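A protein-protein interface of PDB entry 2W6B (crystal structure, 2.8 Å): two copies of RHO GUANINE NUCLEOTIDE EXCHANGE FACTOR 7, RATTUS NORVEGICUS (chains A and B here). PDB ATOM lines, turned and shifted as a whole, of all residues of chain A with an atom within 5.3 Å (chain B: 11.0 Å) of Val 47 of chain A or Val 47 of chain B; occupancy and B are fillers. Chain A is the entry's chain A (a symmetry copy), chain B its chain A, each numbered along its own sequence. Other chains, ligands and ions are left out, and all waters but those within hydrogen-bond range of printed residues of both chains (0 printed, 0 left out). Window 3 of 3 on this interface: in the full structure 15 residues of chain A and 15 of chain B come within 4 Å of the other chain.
Leu 43 of chain B touches its own counterpart, Leu 43 of chain A.
Glu 44 of chain A touches Leu 43 of chain B, but with the chains exchanged Leu 43 of chain A does not touch Glu 44 of chain B (7.4 Å).
Arg 48 of chain A touches Leu 46 of chain B, but with the chains exchanged Leu 46 of chain A does not touch Arg 48 of chain B (11.7 Å).
Leu 51 of chain A touches Val 50 of chain B, but with the chains exchanged Val 50 of chain A does not touch Leu 51 of chain B (7.6 Å).
10 positions are printed for both chains.
Of the 5 pairs that touch across the chains among the printed residues, 2 have their exchanged pair printed and touching as well.
Leu 43 of chain A touches just one residue of chain B: Leu 43 (3.7 Å).
Printed residues of chain B within 4 Å of Glu 44 of chain A: Leu 43.
Val 47 of chain A touches just one residue of chain B: Val 47.
No residue of chain B comes within 4 Å of Val 50 of chain A.
Lys 41 of chain B touches none of the printed residues of chain A.
Of the printed residues of chain A, Leu 43 of chain B touches Leu 43 (3.7 Å) and Glu 44 (3.9 Å).
Of the printed residues of chain A, Leu 46 of chain B touches Arg 48.
Of chain A, only Val 47 comes within 4 Å of Val 47 of chain B.
Printed residues of chain A within 4 Å of Val 50 of chain B: Leu 51 (3.3 Å).
Leu 43 of chain A touches Leu 43 of chain B.
Glu 44 of chain A touches Leu 43 of chain B.
Val 47 of chain A touches Val 47 of chain B (CG2 to CG2, 3.5 Å).
Arg 48 of chain A touches Leu 46 of chain B.
CG2 of Val 50 of chain B touches CD2 of Leu 51 of chain A (3.3 Å).
Of the 17 printed residues of chain B, 4 touch a printed residue of chain A.
Of the 10 printed residues of chain A, 5 touch a printed residue of chain B.
Hydrophobic or aromatic side chains of chain A within 4 Å of the printed part of chain B: Leu 43, Val 47 and Leu 51.
Among the printed residues, 5 pairs touch across the chains.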
ATOM      1  N   LEU A  43     -15.085  34.854  26.313  1.00  0.00           N
ATOM      2  CA  LEU A  43     -15.917  34.338  27.394  1.00  0.00           C
ATOM      3  C   LEU A  43     -16.460  32.976  27.044  1.00  0.00           C
ATOM      4  O   LEU A  43     -16.486  32.086  27.889  1.00  0.00           O
ATOM      5  CB  LEU A  43     -17.081  35.271  27.664  1.00  0.00           C
ATOM      6  CG  LEU A  43     -17.310  35.658  29.124  1.00  0.00           C
ATOM      7  CD1 LEU A  43     -18.785  35.910  29.324  1.00  0.00           C
ATOM      8  CD2 LEU A  43     -16.814  34.586  30.103  1.00  0.00           C
ATOM      9  N   GLU A  44     -16.887  32.811  25.800  1.00  0.00           N
ATOM     10  CA  GLU A  44     -17.250  31.494  25.314  1.00  0.00           C
ATOM     11  C   GLU A  44     -16.121  30.486  25.514  1.00  0.00           C
ATOM     12  O   GLU A  44     -16.370  29.373  25.980  1.00  0.00           O
ATOM     13  CB  GLU A  44     -17.653  31.559  23.858  1.00  0.00           C
ATOM     14  CG  GLU A  44     -19.062  32.033  23.671  1.00  0.00           C
ATOM     15  CD  GLU A  44     -19.248  32.763  22.366  1.00  0.00           C
ATOM     16  OE1 GLU A  44     -18.569  32.391  21.380  1.00  0.00           O
ATOM     17  OE2 GLU A  44     -20.064  33.714  22.319  1.00  0.00           O
ATOM     18  N   LYS A  45     -14.887  30.877  25.185  1.00  0.00           N
ATOM     19  CA  LYS A  45     -13.732  29.993  25.380  1.00  0.00           C
ATOM     20  C   LYS A  45     -13.776  29.483  26.799  1.00  0.00           C
ATOM     21  O   LYS A  45     -13.943  28.290  27.017  1.00  0.00           O
ATOM     22  CB  LYS A  45     -12.391  30.704  25.116  1.00  0.00           C
ATOM     23  CG  LYS A  45     -12.179  31.324  23.704  1.00  0.00           C
ATOM     24  CD  LYS A  45     -12.523  30.368  22.545  1.00  0.00           C
ATOM     25  CE  LYS A  45     -13.940  30.631  21.974  1.00  0.00           C
ATOM     26  NZ  LYS A  45     -14.612  29.399  21.427  1.00  0.00           N
ATOM     27  N   LEU A  46     -13.674  30.411  27.749  1.00  0.00           N
ATOM     28  CA  LEU A  46     -13.774  30.116  29.167  1.00  0.00           C
ATOM     29  C   LEU A  46     -14.938  29.199  29.480  1.00  0.00           C
ATOM     30  O   LEU A  46     -14.744  28.161  30.096  1.00  0.00           O
ATOM     31  CB  LEU A  46     -13.924  31.396  29.977  1.00  0.00           C
ATOM     32  CG  LEU A  46     -12.748  32.355  30.124  1.00  0.00           C
ATOM     33  CD1 LEU A  46     -13.235  33.565  30.901  1.00  0.00           C
ATOM     34  CD2 LEU A  46     -11.582  31.703  30.844  1.00  0.00           C
ATOM     35  N   VAL A  47     -16.142  29.571  29.056  1.00  0.00           N
ATOM     36  CA  VAL A  47     -17.316  28.733  29.302  1.00  0.00           C
ATOM     37  C   VAL A  47     -17.153  27.355  28.687  1.00  0.00           C
ATOM     38  O   VAL A  47     -17.447  26.356  29.335  1.00  0.00           O
ATOM     39  CB  VAL A  47     -18.628  29.398  28.847  1.00  0.00           C
ATOM     40  CG1 VAL A  47     -19.723  28.388  28.652  1.00  0.00           C
ATOM     41  CG2 VAL A  47     -19.060  30.368  29.877  1.00  0.00           C
ATOM     42  N   ARG A  48     -16.659  27.293  27.456  1.00  0.00           N
ATOM     43  CA  ARG A  48     -16.466  26.008  26.791  1.00  0.00           C
ATOM     44  C   ARG A  48     -15.446  25.119  27.505  1.00  0.00           C
ATOM     45  O   ARG A  48     -15.661  23.906  27.619  1.00  0.00           O
ATOM     46  CB  ARG A  48     -16.090  26.200  25.324  1.00  0.00           C
ATOM     47  CG  ARG A  48     -17.289  26.198  24.370  1.00  0.00           C
ATOM     48  CD  ARG A  48     -18.440  27.077  24.864  1.00  0.00           C
ATOM     49  NE  ARG A  48     -19.054  27.834  23.780  1.00  0.00           N
ATOM     50  CZ  ARG A  48     -20.064  27.399  23.035  1.00  0.00           C
ATOM     51  NH1 ARG A  48     -20.587  26.194  23.251  1.00  0.00           N
ATOM     52  NH2 ARG A  48     -20.556  28.174  22.073  1.00  0.00           N
ATOM     53  N   LYS A  49     -14.354  25.727  27.985  1.00  0.00           N
ATOM     54  CA  LYS A  49     -13.374  25.049  28.844  1.00  0.00           C
ATOM     55  C   LYS A  49     -14.029  24.451  30.099  1.00  0.00           C
ATOM     56  O   LYS A  49     -13.684  23.336  30.507  1.00  0.00           O
ATOM     57  CB  LYS A  49     -12.236  25.996  29.238  1.00  0.00           C
ATOM     58  N   VAL A  50     -14.977  25.184  30.694  1.00  0.00           N
ATOM     59  CA  VAL A  50     -15.785  24.679  31.813  1.00  0.00           C
ATOM     60  C   VAL A  50     -16.540  23.401  31.422  1.00  0.00           C
ATOM     61  O   VAL A  50     -16.392  22.372  32.080  1.00  0.00           O
ATOM     62  CB  VAL A  50     -16.785  25.746  32.339  1.00  0.00           C
ATOM     63  CG1 VAL A  50     -17.731  25.144  33.346  1.00  0.00           C
ATOM     64  CG2 VAL A  50     -16.051  26.910  32.960  1.00  0.00           C
ATOM     65  N   LEU A  51     -17.318  23.470  30.340  1.00  0.00           N
ATOM     66  CA  LEU A  51     -18.154  22.348  29.886  1.00  0.00           C
ATOM     67  C   LEU A  51     -17.354  21.086  29.547  1.00  0.00           C
ATOM     68  O   LEU A  51     -17.803  19.956  29.796  1.00  0.00           O
ATOM     69  CB  LEU A  51     -19.009  22.782  28.695  1.00  0.00           C
ATOM     70  CG  LEU A  51     -19.868  24.038  28.912  1.00  0.00           C
ATOM     71  CD1 LEU A  51     -20.627  24.383  27.649  1.00  0.00           C
ATOM     72  CD2 LEU A  51     -20.851  23.849  30.045  1.00  0.00           C
ATOM     73  N   LYS A  52     -16.166  21.301  28.981  1.00  0.00           N
ATOM     74  CA  LYS A  52     -15.202  20.237  28.720  1.00  0.00           C
ATOM     75  C   LYS A  52     -14.256  20.067  29.916  1.00  0.00           C
ATOM     76  O   LYS A  52     -13.107  19.630  29.813  1.00  0.00           O
ATOM     77  CB  LYS A  52     -14.423  20.520  27.426  1.00  0.00           C
ATOM     78  N   ALA B  39     -26.071  36.749  20.632  1.00  0.00           N
ATOM     79  CA  ALA B  39     -24.933  35.889  20.875  1.00  0.00           C
ATOM     80  C   ALA B  39     -24.637  35.728  22.365  1.00  0.00           C
ATOM     81  O   ALA B  39     -24.267  34.641  22.807  1.00  0.00           O
ATOM     82  CB  ALA B  39     -23.743  36.412  20.162  1.00  0.00           C
ATOM     83  N   ARG B  40     -24.811  36.795  23.143  1.00  0.00           N
ATOM     84  CA  ARG B  40     -24.490  36.724  24.561  1.00  0.00           C
ATOM     85  C   ARG B  40     -25.651  36.232  25.394  1.00  0.00           C
ATOM     86  O   ARG B  40     -25.436  35.566  26.399  1.00  0.00           O
ATOM     87  CB  ARG B  40     -23.897  38.037  25.094  1.00  0.00           C
ATOM     88  CG  ARG B  40     -24.870  39.022  25.670  1.00  0.00           C
ATOM     89  CD  ARG B  40     -24.894  39.049  27.193  1.00  0.00           C
ATOM     90  NE  ARG B  40     -25.767  40.137  27.637  1.00  0.00           N
ATOM     91  CZ  ARG B  40     -27.091  40.049  27.765  1.00  0.00           C
ATOM     92  NH1 ARG B  40     -27.712  38.906  27.517  1.00  0.00           N
ATOM     93  NH2 ARG B  40     -27.804  41.102  28.149  1.00  0.00           N
ATOM     94  N   LYS B  41     -26.876  36.549  24.986  1.00  0.00           N
ATOM     95  CA  LYS B  41     -28.046  35.979  25.643  1.00  0.00           C
ATOM     96  C   LYS B  41     -27.992  34.451  25.610  1.00  0.00           C
ATOM     97  O   LYS B  41     -28.301  33.803  26.602  1.00  0.00           O
ATOM     98  CB  LYS B  41     -29.344  36.521  25.046  1.00  0.00           C
ATOM     99  CG  LYS B  41     -30.025  37.563  25.924  1.00  0.00           C
ATOM    100  CD  LYS B  41     -30.798  38.617  25.117  1.00  0.00           C
ATOM    101  CE  LYS B  41     -31.877  39.311  25.979  1.00  0.00           C
ATOM    102  NZ  LYS B  41     -32.074  40.778  25.683  1.00  0.00           N
ATOM    103  N   ASP B  42     -27.552  33.884  24.487  1.00  0.00           N
ATOM    104  CA  ASP B  42     -27.366  32.437  24.365  1.00  0.00           C
ATOM    105  C   ASP B  42     -26.325  31.918  25.337  1.00  0.00           C
ATOM    106  O   ASP B  42     -26.367  30.755  25.740  1.00  0.00           O
ATOM    107  CB  ASP B  42     -26.918  32.059  22.948  1.00  0.00           C
ATOM    108  CG  ASP B  42     -28.010  32.266  21.892  1.00  0.00           C
ATOM    109  OD1 ASP B  42     -29.218  32.217  22.230  1.00  0.00           O
ATOM    110  OD2 ASP B  42     -27.647  32.460  20.705  1.00  0.00           O
ATOM    111  N   LEU B  43     -25.379  32.789  25.686  1.00  0.00           N
ATOM    112  CA  LEU B  43     -24.273  32.446  26.571  1.00  0.00           C
ATOM    113  C   LEU B  43     -24.749  32.320  27.995  1.00  0.00           C
ATOM    114  O   LEU B  43     -24.343  31.405  28.705  1.00  0.00           O
ATOM    115  CB  LEU B  43     -23.191  33.507  26.512  1.00  0.00           C
ATOM    116  CG  LEU B  43     -21.764  33.003  26.305  1.00  0.00           C
ATOM    117  CD1 LEU B  43     -20.817  33.966  26.979  1.00  0.00           C
ATOM    118  CD2 LEU B  43     -21.555  31.582  26.845  1.00  0.00           C
ATOM    119  N   GLU B  44     -25.617  33.233  28.411  1.00  0.00           N
ATOM    120  CA  GLU B  44     -26.276  33.093  29.694  1.00  0.00           C
ATOM    121  C   GLU B  44     -26.981  31.746  29.825  1.00  0.00           C
ATOM    122  O   GLU B  44     -26.850  31.084  30.855  1.00  0.00           O
ATOM    123  CB  GLU B  44     -27.251  34.228  29.917  1.00  0.00           C
ATOM    124  CG  GLU B  44     -26.577  35.483  30.382  1.00  0.00           C
ATOM    125  CD  GLU B  44     -27.312  36.721  29.938  1.00  0.00           C
ATOM    126  OE1 GLU B  44     -28.561  36.667  29.853  1.00  0.00           O
ATOM    127  OE2 GLU B  44     -26.648  37.749  29.664  1.00  0.00           O
ATOM    128  N   LYS B  45     -27.706  31.332  28.781  1.00  0.00           N
ATOM    129  CA  LYS B  45     -28.388  30.033  28.796  1.00  0.00           C
ATOM    130  C   LYS B  45     -27.379  28.987  29.200  1.00  0.00           C
ATOM    131  O   LYS B  45     -27.515  28.376  30.251  1.00  0.00           O
ATOM    132  CB  LYS B  45     -29.006  29.674  27.432  1.00  0.00           C
ATOM    133  CG  LYS B  45     -30.053  30.661  26.841  1.00  0.00           C
ATOM    134  CD  LYS B  45     -31.151  31.078  27.839  1.00  0.00           C
ATOM    135  CE  LYS B  45     -30.857  32.455  28.488  1.00  0.00           C
ATOM    136  NZ  LYS B  45     -31.391  32.591  29.889  1.00  0.00           N
ATOM    137  N   LEU B  46     -26.346  28.835  28.372  1.00  0.00           N
ATOM    138  CA  LEU B  46     -25.239  27.933  28.637  1.00  0.00           C
ATOM    139  C   LEU B  46     -24.734  28.048  30.060  1.00  0.00           C
ATOM    140  O   LEU B  46     -24.667  27.049  30.762  1.00  0.00           O
ATOM    141  CB  LEU B  46     -24.084  28.199  27.681  1.00  0.00           C
ATOM    142  CG  LEU B  46     -24.206  27.831  26.206  1.00  0.00           C
ATOM    143  CD1 LEU B  46     -22.941  28.298  25.509  1.00  0.00           C
ATOM    144  CD2 LEU B  46     -24.388  26.336  26.017  1.00  0.00           C
ATOM    145  N   VAL B  47     -24.385  29.257  30.490  1.00  0.00           N
ATOM    146  CA  VAL B  47     -23.903  29.457  31.858  1.00  0.00           C
ATOM    147  C   VAL B  47     -24.937  29.020  32.880  1.00  0.00           C
ATOM    148  O   VAL B  47     -24.599  28.339  33.841  1.00  0.00           O
ATOM    149  CB  VAL B  47     -23.431  30.898  32.117  1.00  0.00           C
ATOM    150  CG1 VAL B  47     -23.404  31.217  33.586  1.00  0.00           C
ATOM    151  CG2 VAL B  47     -22.065  31.065  31.574  1.00  0.00           C
ATOM    152  N   ARG B  48     -26.196  29.381  32.662  1.00  0.00           N
ATOM    153  CA  ARG B  48     -27.255  29.001  33.592  1.00  0.00           C
ATOM    154  C   ARG B  48     -27.451  27.487  33.679  1.00  0.00           C
ATOM    155  O   ARG B  48     -27.657  26.956  34.779  1.00  0.00           O
ATOM    156  CB  ARG B  48     -28.567  29.702  33.247  1.00  0.00           C
ATOM    157  CG  ARG B  48     -28.777  31.028  33.987  1.00  0.00           C
ATOM    158  CD  ARG B  48     -27.536  31.924  33.958  1.00  0.00           C
ATOM    159  NE  ARG B  48     -27.878  33.324  33.742  1.00  0.00           N
ATOM    160  CZ  ARG B  48     -28.151  34.192  34.711  1.00  0.00           C
ATOM    161  NH1 ARG B  48     -28.124  33.805  35.985  1.00  0.00           N
ATOM    162  NH2 ARG B  48     -28.446  35.451  34.405  1.00  0.00           N
ATOM    163  N   LYS B  49     -27.378  26.806  32.529  1.00  0.00           N
ATOM    164  CA  LYS B  49     -27.366  25.338  32.467  1.00  0.00           C
ATOM    165  C   LYS B  49     -26.229  24.739  33.310  1.00  0.00           C
ATOM    166  O   LYS B  49     -26.428  23.724  33.988  1.00  0.00           O
ATOM    167  CB  LYS B  49     -27.272  24.846  31.020  1.00  0.00           C
ATOM    168  N   VAL B  50     -25.051  25.373  33.274  1.00  0.00           N
ATOM    169  CA  VAL B  50     -23.922  24.997  34.137  1.00  0.00           C
ATOM    170  C   VAL B  50     -24.304  25.075  35.621  1.00  0.00           C
ATOM    171  O   VAL B  50     -24.177  24.086  36.343  1.00  0.00           O
ATOM    172  CB  VAL B  50     -22.665  25.870  33.865  1.00  0.00           C
ATOM    173  CG1 VAL B  50     -21.594  25.600  34.891  1.00  0.00           C
ATOM    174  CG2 VAL B  50     -22.122  25.616  32.480  1.00  0.00           C
ATOM    175  N   LEU B  51     -24.794  26.237  36.055  1.00  0.00           N
ATOM    176  CA  LEU B  51     -25.138  26.482  37.464  1.00  0.00           C
ATOM    177  C   LEU B  51     -26.212  25.532  38.006  1.00  0.00           C
ATOM    178  O   LEU B  51     -26.168  25.116  39.175  1.00  0.00           O
ATOM    179  CB  LEU B  51     -25.560  27.939  37.654  1.00  0.00           C
ATOM    180  CG  LEU B  51     -24.560  28.994  37.155  1.00  0.00           C
ATOM    181  CD1 LEU B  51     -25.116  30.386  37.359  1.00  0.00           C
ATOM    182  CD2 LEU B  51     -23.232  28.881  37.867  1.00  0.00           C
ATOM    183  N   LYS B  52     -27.166  25.198  37.137  1.00  0.00           N
ATOM    184  CA  LYS B  52     -28.189  24.196  37.422  1.00  0.00           C
ATOM    185  C   LYS B  52     -27.718  22.809  36.965  1.00  0.00           C
ATOM    186  O   LYS B  52     -28.493  21.907  36.632  1.00  0.00           O
ATOM    187  CB  LYS B  52     -29.520  24.582  36.760  1.00  0.00           C
ATOM    188  N   ASN B  53     -26.353  22.630  37.029  1.00  0.00           N
ATOM    189  CA  ASN B  53     -25.798  21.284  36.946  1.00  0.00           C
ATOM    190  C   ASN B  53     -25.033  21.018  38.248  1.00  0.00           C
ATOM    191  O   ASN B  53     -24.894  19.870  38.686  1.00  0.00           O
ATOM    192  CB  ASN B  53     -24.895  21.116  35.712  1.00  0.00           C
ATOM    193  N   MET B  54     -24.573  22.103  38.878  1.00  0.00           N
ATOM    194  CA  MET B  54     -23.939  22.040  40.194  1.00  0.00           C
ATOM    195  C   MET B  54     -24.973  21.985  41.296  1.00  0.00           C
ATOM    196  O   MET B  54     -25.193  20.927  41.899  1.00  0.00           O
ATOM    197  CB  MET B  54     -23.016  23.226  40.395  1.00  0.00           C
ATOM    198  CG  MET B  54     -21.663  22.968  39.809  1.00  0.00           C
ATOM    199  SD  MET B  54     -21.137  24.500  38.761  1.00  0.00           S
ATOM    200  CE  MET B  54     -20.911  25.837  40.246  1.00  0.00           C
ATOM    201  N   ASN B  55     -25.670  23.107  41.570  1.00  0.00           N
ATOM    202  CA  ASN B  55     -26.784  23.088  42.514  1.00  0.00           C
ATOM    203  C   ASN B  55     -28.075  22.633  41.806  1.00  0.00           C
ATOM    204  O   ASN B  55     -28.905  23.463  41.397  1.00  0.00           O
ATOM    205  CB  ASN B  55     -26.948  24.444  43.209  1.00  0.00           C
